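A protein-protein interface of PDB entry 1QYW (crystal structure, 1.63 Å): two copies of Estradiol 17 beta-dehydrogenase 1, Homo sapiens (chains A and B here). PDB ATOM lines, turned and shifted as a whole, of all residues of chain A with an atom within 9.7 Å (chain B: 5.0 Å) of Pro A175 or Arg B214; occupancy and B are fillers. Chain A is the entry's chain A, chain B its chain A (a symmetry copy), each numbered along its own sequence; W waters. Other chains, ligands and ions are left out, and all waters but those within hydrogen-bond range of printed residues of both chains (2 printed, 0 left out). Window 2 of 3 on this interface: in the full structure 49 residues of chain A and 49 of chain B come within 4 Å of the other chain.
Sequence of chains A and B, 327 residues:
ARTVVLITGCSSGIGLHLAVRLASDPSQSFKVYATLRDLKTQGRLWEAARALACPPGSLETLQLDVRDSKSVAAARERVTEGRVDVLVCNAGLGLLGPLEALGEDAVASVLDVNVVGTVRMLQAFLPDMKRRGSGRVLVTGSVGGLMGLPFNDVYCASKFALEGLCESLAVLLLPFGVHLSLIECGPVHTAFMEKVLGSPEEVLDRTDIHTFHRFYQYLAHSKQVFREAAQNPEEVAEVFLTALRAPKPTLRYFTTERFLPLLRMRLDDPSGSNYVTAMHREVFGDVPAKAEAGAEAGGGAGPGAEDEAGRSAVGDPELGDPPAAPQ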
ATOM      1  N   MET A 129      -7.298  19.824 -27.842  1.00  0.00           N
ATOM      2  CA  MET A 129      -6.622  21.065 -27.504  1.00  0.00           C
ATOM      3  C   MET A 129      -7.233  21.667 -26.242  1.00  0.00           C
ATOM      4  O   MET A 129      -6.575  22.221 -25.354  1.00  0.00           O
ATOM      5  CB  MET A 129      -6.723  22.051 -28.679  1.00  0.00           C
ATOM      6  CG  MET A 129      -5.930  21.561 -29.873  1.00  0.00           C
ATOM      7  SD  MET A 129      -5.945  22.820 -31.197  1.00  0.00           S
ATOM      8  CE  MET A 129      -4.901  22.019 -32.389  1.00  0.00           C
ATOM      9  N   LYS A 130      -8.568  21.636 -26.178  1.00  0.00           N
ATOM     10  CA  LYS A 130      -9.280  22.199 -25.029  1.00  0.00           C
ATOM     11  C   LYS A 130      -8.909  21.448 -23.750  1.00  0.00           C
ATOM     12  O   LYS A 130      -8.687  22.073 -22.718  1.00  0.00           O
ATOM     13  CB  LYS A 130     -10.787  22.155 -25.276  1.00  0.00           C
ATOM     14  CG  LYS A 130     -11.228  23.183 -26.314  1.00  0.00           C
ATOM     15  CD  LYS A 130     -12.664  22.902 -26.753  1.00  0.00           C
ATOM     16  CE  LYS A 130     -13.664  23.874 -26.169  1.00  0.00           C
ATOM     17  NZ  LYS A 130     -15.080  23.489 -26.453  1.00  0.00           N
ATOM     18  N   ARG A 132      -6.121  19.746 -23.124  1.00  0.00           N
ATOM     19  CA  ARG A 132      -4.727  20.034 -22.802  1.00  0.00           C
ATOM     20  C   ARG A 132      -4.493  21.478 -22.405  1.00  0.00           C
ATOM     21  O   ARG A 132      -3.543  21.847 -21.702  1.00  0.00           O
ATOM     22  CB  ARG A 132      -3.865  19.644 -23.998  1.00  0.00           C
ATOM     23  CG  ARG A 132      -2.396  20.002 -23.867  1.00  0.00           C
ATOM     24  CD  ARG A 132      -1.638  19.666 -25.143  1.00  0.00           C
ATOM     25  NE  ARG A 132      -2.391  20.036 -26.341  1.00  0.00           N
ATOM     26  CZ  ARG A 132      -1.832  20.228 -27.532  1.00  0.00           C
ATOM     27  NH1 ARG A 132      -0.512  20.084 -27.667  1.00  0.00           N
ATOM     28  NH2 ARG A 132      -2.580  20.560 -28.581  1.00  0.00           N
ATOM     29  N   GLY A 133      -5.350  22.358 -22.908  1.00  0.00           N
ATOM     30  CA  GLY A 133      -5.287  23.778 -22.641  1.00  0.00           C
ATOM     31  C   GLY A 133      -4.195  24.407 -23.504  1.00  0.00           C
ATOM     32  O   GLY A 133      -3.593  25.391 -23.084  1.00  0.00           O
ATOM     33  N   SER A 134      -3.971  23.821 -24.687  1.00  0.00           N
ATOM     34  CA  SER A 134      -2.957  24.394 -25.563  1.00  0.00           C
ATOM     35  C   SER A 134      -3.176  23.945 -27.010  1.00  0.00           C
ATOM     36  O   SER A 134      -3.729  22.885 -27.281  1.00  0.00           O
ATOM     37  CB  SER A 134      -1.543  24.065 -25.094  1.00  0.00           C
ATOM     38  OG  SER A 134      -1.111  22.804 -25.571  1.00  0.00           O
ATOM     39  N   SER A 168     -16.835  33.565 -33.488  1.00  0.00           N
ATOM     40  CA  SER A 168     -17.718  32.940 -32.508  1.00  0.00           C
ATOM     41  C   SER A 168     -16.948  31.998 -31.604  1.00  0.00           C
ATOM     42  O   SER A 168     -17.040  32.084 -30.364  1.00  0.00           O
ATOM     43  CB  SER A 168     -18.891  32.180 -33.173  1.00  0.00           C
ATOM     44  OG  SER A 168     -19.675  33.079 -33.939  1.00  0.00           O
ATOM     45  N   LEU A 169     -16.119  31.138 -32.203  1.00  0.00           N
ATOM     46  CA  LEU A 169     -15.278  30.233 -31.412  1.00  0.00           C
ATOM     47  C   LEU A 169     -14.257  30.981 -30.592  1.00  0.00           C
ATOM     48  O   LEU A 169     -14.051  30.603 -29.403  1.00  0.00           O
ATOM     49  CB  LEU A 169     -14.560  29.305 -32.394  1.00  0.00           C
ATOM     50  CG  LEU A 169     -15.441  28.202 -32.954  1.00  0.00           C
ATOM     51  CD1 LEU A 169     -14.778  27.554 -34.165  1.00  0.00           C
ATOM     52  CD2 LEU A 169     -15.679  27.170 -31.861  1.00  0.00           C
ATOM     53  N   ALA A 170     -13.640  32.041 -31.103  1.00  0.00           N
ATOM     54  CA  ALA A 170     -12.641  32.800 -30.351  1.00  0.00           C
ATOM     55  C   ALA A 170     -13.220  33.352 -29.047  1.00  0.00           C
ATOM     56  O   ALA A 170     -12.509  33.433 -28.049  1.00  0.00           O
ATOM     57  CB  ALA A 170     -12.058  33.967 -31.125  1.00  0.00           C
ATOM     58  N   VAL A 171     -14.473  33.823 -29.112  1.00  0.00           N
ATOM     59  CA  VAL A 171     -15.099  34.360 -27.892  1.00  0.00           C
ATOM     60  C   VAL A 171     -15.126  33.282 -26.820  1.00  0.00           C
ATOM     61  O   VAL A 171     -14.845  33.593 -25.653  1.00  0.00           O
ATOM     62  CB  VAL A 171     -16.497  34.901 -28.216  1.00  0.00           C
ATOM     63  CG1 VAL A 171     -17.212  35.379 -26.948  1.00  0.00           C
ATOM     64  CG2 VAL A 171     -16.401  36.086 -29.179  1.00  0.00           C
ATOM     65  N   LEU A 172     -15.490  32.045 -27.168  1.00  0.00           N
ATOM     66  CA  LEU A 172     -15.509  30.988 -26.171  1.00  0.00           C
ATOM     67  C   LEU A 172     -14.116  30.527 -25.771  1.00  0.00           C
ATOM     68  O   LEU A 172     -13.816  30.326 -24.590  1.00  0.00           O
ATOM     69  CB  LEU A 172     -16.305  29.777 -26.663  1.00  0.00           C
ATOM     70  CG  LEU A 172     -16.160  28.515 -25.810  1.00  0.00           C
ATOM     71  CD1 LEU A 172     -16.810  28.730 -24.432  1.00  0.00           C
ATOM     72  CD2 LEU A 172     -16.762  27.311 -26.508  1.00  0.00           C
ATOM     73  N   LEU A 173     -13.231  30.352 -26.755  1.00  0.00           N
ATOM     74  CA  LEU A 173     -11.909  29.804 -26.490  1.00  0.00           C
ATOM     75  C   LEU A 173     -10.927  30.696 -25.754  1.00  0.00           C
ATOM     76  O   LEU A 173      -9.894  30.180 -25.303  1.00  0.00           O
ATOM     77  CB  LEU A 173     -11.304  29.346 -27.822  1.00  0.00           C
ATOM     78  CG  LEU A 173     -11.950  28.186 -28.578  1.00  0.00           C
ATOM     79  CD1 LEU A 173     -11.260  28.006 -29.936  1.00  0.00           C
ATOM     80  CD2 LEU A 173     -11.899  26.879 -27.791  1.00  0.00           C
ATOM     81  N   LEU A 174     -11.203  31.958 -25.521  1.00  0.00           N
ATOM     82  CA  LEU A 174     -10.344  32.941 -24.888  1.00  0.00           C
ATOM     83  C   LEU A 174      -9.638  32.446 -23.636  1.00  0.00           C
ATOM     84  O   LEU A 174      -8.404  32.410 -23.641  1.00  0.00           O
ATOM     85  CB  LEU A 174     -11.100  34.251 -24.681  1.00  0.00           C
ATOM     86  CG  LEU A 174     -10.337  35.467 -24.158  1.00  0.00           C
ATOM     87  CD1 LEU A 174      -9.162  35.818 -25.061  1.00  0.00           C
ATOM     88  CD2 LEU A 174     -11.253  36.682 -24.017  1.00  0.00           C
ATOM     89  N   PRO A 175     -10.357  31.972 -22.630  1.00  0.00           N
ATOM     90  CA  PRO A 175      -9.780  31.423 -21.417  1.00  0.00           C
ATOM     91  C   PRO A 175      -9.322  29.973 -21.465  1.00  0.00           C
ATOM     92  O   PRO A 175      -8.805  29.464 -20.454  1.00  0.00           O
ATOM     93  CB  PRO A 175     -10.929  31.538 -20.406  1.00  0.00           C
ATOM     94  CG  PRO A 175     -12.180  31.462 -21.212  1.00  0.00           C
ATOM     95  CD  PRO A 175     -11.843  32.019 -22.569  1.00  0.00           C
ATOM     96  N   PHE A 176      -9.477  29.230 -22.564  1.00  0.00           N
ATOM     97  CA  PHE A 176      -9.072  27.828 -22.612  1.00  0.00           C
ATOM     98  C   PHE A 176      -7.595  27.620 -22.934  1.00  0.00           C
ATOM     99  O   PHE A 176      -7.100  26.485 -22.853  1.00  0.00           O
ATOM    100  CB  PHE A 176      -9.884  27.034 -23.646  1.00  0.00           C
ATOM    101  CG  PHE A 176     -11.253  26.576 -23.247  1.00  0.00           C
ATOM    102  CD1 PHE A 176     -12.325  27.456 -23.275  1.00  0.00           C
ATOM    103  CD2 PHE A 176     -11.484  25.263 -22.872  1.00  0.00           C
ATOM    104  CE1 PHE A 176     -13.597  27.045 -22.916  1.00  0.00           C
ATOM    105  CE2 PHE A 176     -12.757  24.841 -22.516  1.00  0.00           C
ATOM    106  CZ  PHE A 176     -13.812  25.732 -22.544  1.00  0.00           C
ATOM    107  N   GLY A 177      -6.894  28.652 -23.380  1.00  0.00           N
ATOM    108  CA  GLY A 177      -5.482  28.476 -23.772  1.00  0.00           C
ATOM    109  C   GLY A 177      -5.325  28.009 -25.229  1.00  0.00           C
ATOM    110  O   GLY A 177      -4.221  27.720 -25.686  1.00  0.00           O
ATOM    111  N   VAL A 178      -6.429  27.873 -25.953  1.00  0.00           N
ATOM    112  CA  VAL A 178      -6.387  27.425 -27.358  1.00  0.00           C
ATOM    113  C   VAL A 178      -6.518  28.705 -28.166  1.00  0.00           C
ATOM    114  O   VAL A 178      -7.406  29.493 -27.847  1.00  0.00           O
ATOM    115  CB  VAL A 178      -7.497  26.426 -27.663  1.00  0.00           C
ATOM    116  CG1 VAL A 178      -7.461  25.942 -29.114  1.00  0.00           C
ATOM    117  CG2 VAL A 178      -7.331  25.193 -26.773  1.00  0.00           C
ATOM    118  N   HIS A 179      -5.642  28.942 -29.132  1.00  0.00           N
ATOM    119  CA  HIS A 179      -5.632  30.205 -29.850  1.00  0.00           C
ATOM    120  C   HIS A 179      -5.983  30.033 -31.317  1.00  0.00           C
ATOM    121  O   HIS A 179      -5.359  29.205 -31.961  1.00  0.00           O
ATOM    122  CB  HIS A 179      -4.212  30.791 -29.735  1.00  0.00           C
ATOM    123  CG  HIS A 179      -3.806  31.001 -28.302  1.00  0.00           C
ATOM    124  ND1 HIS A 179      -3.023  30.120 -27.606  1.00  0.00           N
ATOM    125  CD2 HIS A 179      -4.112  32.015 -27.458  1.00  0.00           C
ATOM    126  CE1 HIS A 179      -2.849  30.587 -26.376  1.00  0.00           C
ATOM    127  NE2 HIS A 179      -3.488  31.738 -26.262  1.00  0.00           N
ATOM    128  N   PHE B 151     -21.245  29.924 -28.932  1.00  0.00           N
ATOM    129  CA  PHE B 151     -22.163  28.812 -29.018  1.00  0.00           C
ATOM    130  C   PHE B 151     -23.186  28.919 -30.147  1.00  0.00           C
ATOM    131  O   PHE B 151     -24.108  28.133 -30.299  1.00  0.00           O
ATOM    132  CB  PHE B 151     -22.918  28.582 -27.675  1.00  0.00           C
ATOM    133  CG  PHE B 151     -21.974  28.196 -26.548  1.00  0.00           C
ATOM    134  CD1 PHE B 151     -21.394  26.949 -26.546  1.00  0.00           C
ATOM    135  CD2 PHE B 151     -21.674  29.116 -25.558  1.00  0.00           C
ATOM    136  CE1 PHE B 151     -20.519  26.586 -25.516  1.00  0.00           C
ATOM    137  CE2 PHE B 151     -20.784  28.754 -24.537  1.00  0.00           C
ATOM    138  CZ  PHE B 151     -20.195  27.513 -24.544  1.00  0.00           C
ATOM    139  N   HIS B 210     -16.246  22.033 -18.582  1.00  0.00           N
ATOM    140  CA  HIS B 210     -15.989  23.457 -18.594  1.00  0.00           C
ATOM    141  C   HIS B 210     -16.789  24.114 -19.733  1.00  0.00           C
ATOM    142  O   HIS B 210     -17.456  25.114 -19.505  1.00  0.00           O
ATOM    143  CB  HIS B 210     -14.500  23.768 -18.770  1.00  0.00           C
ATOM    144  CG  HIS B 210     -13.709  22.984 -17.754  1.00  0.00           C
ATOM    145  ND1 HIS B 210     -13.823  23.240 -16.400  1.00  0.00           N
ATOM    146  CD2 HIS B 210     -12.826  21.974 -17.895  1.00  0.00           C
ATOM    147  CE1 HIS B 210     -13.025  22.408 -15.750  1.00  0.00           C
ATOM    148  NE2 HIS B 210     -12.415  21.635 -16.634  1.00  0.00           N
ATOM    149  N   THR B 211     -16.740  23.482 -20.911  1.00  0.00           N
ATOM    150  CA  THR B 211     -17.549  24.032 -22.012  1.00  0.00           C
ATOM    151  C   THR B 211     -19.034  23.946 -21.671  1.00  0.00           C
ATOM    152  O   THR B 211     -19.790  24.897 -21.924  1.00  0.00           O
ATOM    153  CB  THR B 211     -17.277  23.307 -23.341  1.00  0.00           C
ATOM    154  OG1 THR B 211     -15.873  23.426 -23.625  1.00  0.00           O
ATOM    155  CG2 THR B 211     -18.094  23.991 -24.431  1.00  0.00           C
ATOM    156  N   PHE B 212     -19.452  22.861 -21.051  1.00  0.00           N
ATOM    157  CA  PHE B 212     -20.837  22.670 -20.620  1.00  0.00           C
ATOM    158  C   PHE B 212     -21.257  23.795 -19.684  1.00  0.00           C
ATOM    159  O   PHE B 212     -22.323  24.425 -19.826  1.00  0.00           O
ATOM    160  CB  PHE B 212     -21.092  21.299 -20.014  1.00  0.00           C
ATOM    161  CG  PHE B 212     -22.517  21.036 -19.644  1.00  0.00           C
ATOM    162  CD1 PHE B 212     -23.396  20.466 -20.550  1.00  0.00           C
ATOM    163  CD2 PHE B 212     -23.003  21.382 -18.386  1.00  0.00           C
ATOM    164  CE1 PHE B 212     -24.716  20.227 -20.207  1.00  0.00           C
ATOM    165  CE2 PHE B 212     -24.320  21.152 -18.046  1.00  0.00           C
ATOM    166  CZ  PHE B 212     -25.184  20.572 -18.958  1.00  0.00           C
ATOM    167  N   HIS B 213     -20.452  24.106 -18.676  1.00  0.00           N
ATOM    168  CA  HIS B 213     -20.721  25.187 -17.737  1.00  0.00           C
ATOM    169  C   HIS B 213     -20.792  26.547 -18.413  1.00  0.00           C
ATOM    170  O   HIS B 213     -21.659  27.382 -18.119  1.00  0.00           O
ATOM    171  CB  HIS B 213     -19.629  25.175 -16.665  1.00  0.00           C
ATOM    172  CG  HIS B 213     -19.620  26.397 -15.795  1.00  0.00           C
ATOM    173  ND1 HIS B 213     -20.310  26.515 -14.613  1.00  0.00           N
ATOM    174  CD2 HIS B 213     -18.957  27.567 -15.968  1.00  0.00           C
ATOM    175  CE1 HIS B 213     -20.061  27.707 -14.103  1.00  0.00           C
ATOM    176  NE2 HIS B 213     -19.262  28.373 -14.906  1.00  0.00           N
ATOM    177  N   ARG B 214     -19.911  26.811 -19.379  1.00  0.00           N
ATOM    178  CA  ARG B 214     -19.915  28.076 -20.102  1.00  0.00           C
ATOM    179  C   ARG B 214     -21.198  28.162 -20.945  1.00  0.00           C
ATOM    180  O   ARG B 214     -21.746  29.252 -21.108  1.00  0.00           O
ATOM    181  CB  ARG B 214     -18.699  28.210 -21.014  1.00  0.00           C
ATOM    182  CG  ARG B 214     -17.392  28.504 -20.297  1.00  0.00           C
ATOM    183  CD  ARG B 214     -17.411  29.813 -19.536  1.00  0.00           C
ATOM    184  NE  ARG B 214     -16.045  30.212 -19.166  1.00  0.00           N
ATOM    185  CZ  ARG B 214     -15.771  31.267 -18.406  1.00  0.00           C
ATOM    186  NH1 ARG B 214     -16.744  32.018 -17.902  1.00  0.00           N
ATOM    187  NH2 ARG B 214     -14.499  31.561 -18.136  1.00  0.00           N
ATOM    188  N   PHE B 215     -21.673  27.031 -21.452  1.00  0.00           N
ATOM    189  CA  PHE B 215     -22.913  27.006 -22.231  1.00  0.00           C
ATOM    190  C   PHE B 215     -24.081  27.437 -21.364  1.00  0.00           C
ATOM    191  O   PHE B 215     -24.928  28.229 -21.786  1.00  0.00           O
ATOM    192  CB  PHE B 215     -23.128  25.649 -22.887  1.00  0.00           C
ATOM    193  CG  PHE B 215     -24.311  25.516 -23.816  1.00  0.00           C
ATOM    194  CD1 PHE B 215     -24.590  26.527 -24.730  1.00  0.00           C
ATOM    195  CD2 PHE B 215     -25.071  24.369 -23.848  1.00  0.00           C
ATOM    196  CE1 PHE B 215     -25.675  26.379 -25.593  1.00  0.00           C
ATOM    197  CE2 PHE B 215     -26.153  24.223 -24.704  1.00  0.00           C
ATOM    198  CZ  PHE B 215     -26.446  25.241 -25.614  1.00  0.00           C
ATOM    199  N   TYR B 216     -24.116  26.906 -20.120  1.00  0.00           N
ATOM    200  CA  TYR B 216     -25.159  27.341 -19.167  1.00  0.00           C
ATOM    201  C   TYR B 216     -25.097  28.837 -18.959  1.00  0.00           C
ATOM    202  O   TYR B 216     -26.133  29.512 -18.912  1.00  0.00           O
ATOM    203  CB  TYR B 216     -24.895  26.718 -17.774  1.00  0.00           C
ATOM    204  CG  TYR B 216     -25.818  27.219 -16.676  1.00  0.00           C
ATOM    205  CD1 TYR B 216     -25.556  28.369 -15.942  1.00  0.00           C
ATOM    206  CD2 TYR B 216     -26.964  26.498 -16.384  1.00  0.00           C
ATOM    207  CE1 TYR B 216     -26.414  28.811 -14.952  1.00  0.00           C
ATOM    208  CE2 TYR B 216     -27.832  26.929 -15.388  1.00  0.00           C
ATOM    209  CZ  TYR B 216     -27.552  28.080 -14.686  1.00  0.00           C
ATOM    210  OH  TYR B 216     -28.424  28.480 -13.697  1.00  0.00           O
ATOM    211  N   GLN B 217     -23.904  29.395 -18.774  1.00  0.00           N
ATOM    212  CA  GLN B 217     -23.727  30.819 -18.548  1.00  0.00           C
ATOM    213  C   GLN B 217     -24.232  31.637 -19.750  1.00  0.00           C
ATOM    214  O   GLN B 217     -24.903  32.664 -19.603  1.00  0.00           O
ATOM    215  CB  GLN B 217     -22.268  31.189 -18.334  1.00  0.00           C
ATOM    216  CG  GLN B 217     -21.657  30.769 -17.014  1.00  0.00           C
ATOM    217  CD  GLN B 217     -20.243  31.282 -16.843  1.00  0.00           C
ATOM    218  OE1 GLN B 217     -19.464  31.376 -17.791  1.00  0.00           O
ATOM    219  NE2 GLN B 217     -19.876  31.624 -15.610  1.00  0.00           N
ATOM    220  N   TYR B 218     -23.898  31.140 -20.935  1.00  0.00           N
ATOM    221  CA  TYR B 218     -24.353  31.781 -22.174  1.00  0.00           C
ATOM    222  C   TYR B 218     -25.882  31.800 -22.186  1.00  0.00           C
ATOM    223  O   TYR B 218     -26.496  32.825 -22.492  1.00  0.00           O
ATOM    224  CB  TYR B 218     -23.764  31.091 -23.434  1.00  0.00           C
ATOM    225  CG  TYR B 218     -24.572  31.532 -24.659  1.00  0.00           C
ATOM    226  CD1 TYR B 218     -24.281  32.708 -25.322  1.00  0.00           C
ATOM    227  CD2 TYR B 218     -25.653  30.754 -25.054  1.00  0.00           C
ATOM    228  CE1 TYR B 218     -25.067  33.103 -26.402  1.00  0.00           C
ATOM    229  CE2 TYR B 218     -26.445  31.155 -26.121  1.00  0.00           C
ATOM    230  CZ  TYR B 218     -26.137  32.319 -26.774  1.00  0.00           C
ATOM    231  OH  TYR B 218     -26.941  32.725 -27.825  1.00  0.00           O
ATOM    232  N   HIS B 280     -16.634  38.560 -24.716  1.00  0.00           N
ATOM    233  CA  HIS B 280     -16.441  37.526 -23.712  1.00  0.00           C
ATOM    234  C   HIS B 280     -16.898  38.057 -22.340  1.00  0.00           C
ATOM    235  O   HIS B 280     -17.579  37.339 -21.604  1.00  0.00           O
ATOM    236  CB  HIS B 280     -14.980  37.099 -23.598  1.00  0.00           C
ATOM    237  CG  HIS B 280     -14.828  35.920 -22.698  1.00  0.00           C
ATOM    238  ND1 HIS B 280     -14.689  36.055 -21.323  1.00  0.00           N
ATOM    239  CD2 HIS B 280     -14.791  34.598 -22.952  1.00  0.00           C
ATOM    240  CE1 HIS B 280     -14.592  34.859 -20.780  1.00  0.00           C
ATOM    241  NE2 HIS B 280     -14.652  33.952 -21.748  1.00  0.00           N
ATOM    242  N   PHE B 284     -20.018  36.382 -20.527  1.00  0.00           N
ATOM    243  CA  PHE B 284     -19.527  35.637 -19.370  1.00  0.00           C
ATOM    244  C   PHE B 284     -19.105  36.535 -18.219  1.00  0.00           C
ATOM    245  O   PHE B 284     -19.457  37.730 -18.237  1.00  0.00           O
ATOM    246  CB  PHE B 284     -18.368  34.744 -19.832  1.00  0.00           C
ATOM    247  CG  PHE B 284     -18.702  33.812 -20.966  1.00  0.00           C
ATOM    248  CD1 PHE B 284     -19.544  32.730 -20.770  1.00  0.00           C
ATOM    249  CD2 PHE B 284     -18.168  34.015 -22.237  1.00  0.00           C
ATOM    250  CE1 PHE B 284     -19.859  31.863 -21.793  1.00  0.00           C
ATOM    251  CE2 PHE B 284     -18.495  33.150 -23.259  1.00  0.00           C
ATOM    252  CZ  PHE B 284     -19.342  32.068 -23.062  1.00  0.00           C
HETATM  253  O   HOH W   1     -18.477  29.457 -29.632  1.00  0.00           O
HETATM  254  O   HOH W   2     -15.041  30.978 -22.183  1.00  0.00           O
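Of the 17 printed residues of chain A, 6 touch a printed residue of chain B. Hydrophobic or aromatic side chains of chain A within 4 Å of the printed part of chain B: Val A171, Leu A172, Leu A174, Pro A175 and Phe A176. Hydrophobic or aromatic side chains of chain B that line the printed part of chain A: Phe B151 and His B280. Among the printed residues, 8 pairs touch across the chains. Among the printed residues, no Asp or Glu carboxylate lies within 4 Å of a Lys or Arg side-chain nitrogen of the other chain.
The guanidinium group (NH1) of Arg B214 is in hydrogen-bond range of the side-chain amide oxygen (OE1) of Gln B217 (2.8 Å).
Ala A170 touches none of the printed residues of chain B. Of the printed residues of chain B, Val A171 touches His B280. Of chain B, only Arg B214 and His B280 come within 4 Å of Pro A175. Printed residues of chain B within 4 Å of Phe A176: Thr B211. Val A178 touches none of the printed residues of chain B. No residue of chain A comes within 4 Å of His B213. Arg B214 touches two residues of chain A. Gln B217 touches none of the printed residues of chain A. The nearest printed residue of chain B that does not touch Pro A175 is Phe B284 (6.6 Å). The nearest residue of chain A that does not touch Arg B214 is Phe A176 (4.8 Å).
The side-chain amino group of Lys A130 is in hydrogen-bond range of the side-chain hydroxyl of Thr B211 (2.9 Å).
Water W2 lies within hydrogen-bond range of the backbone carbonyl oxygen of Leu A172 (2.8 Å), a ring nitrogen (NE2) of His B280 (3.0 Å) and the guanidinium group of Arg B214 (3.3 Å). Water W1 lies within hydrogen-bond range of the backbone NH (N) of Phe B151 (2.9 Å) and the backbone carbonyl oxygen (O) of Ser A168 (3.1 Å).
O of Val A171 touches CD2 of His B280, at 2.9 Å. Phe B151 touches Leu A172 (CZ to CD1, 3.6 Å). CD1 of Leu A172 touches CB of Arg B214, at 3.9 Å. His B280 touches Leu A174. Arg B214 touches Pro A175. NE2 of His B280 touches CD of Pro A175, 3.5 Å away. Thr B211 touches Phe A176 (OG1 to CZ, 3.3 Å).
No position is printed for both chains.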
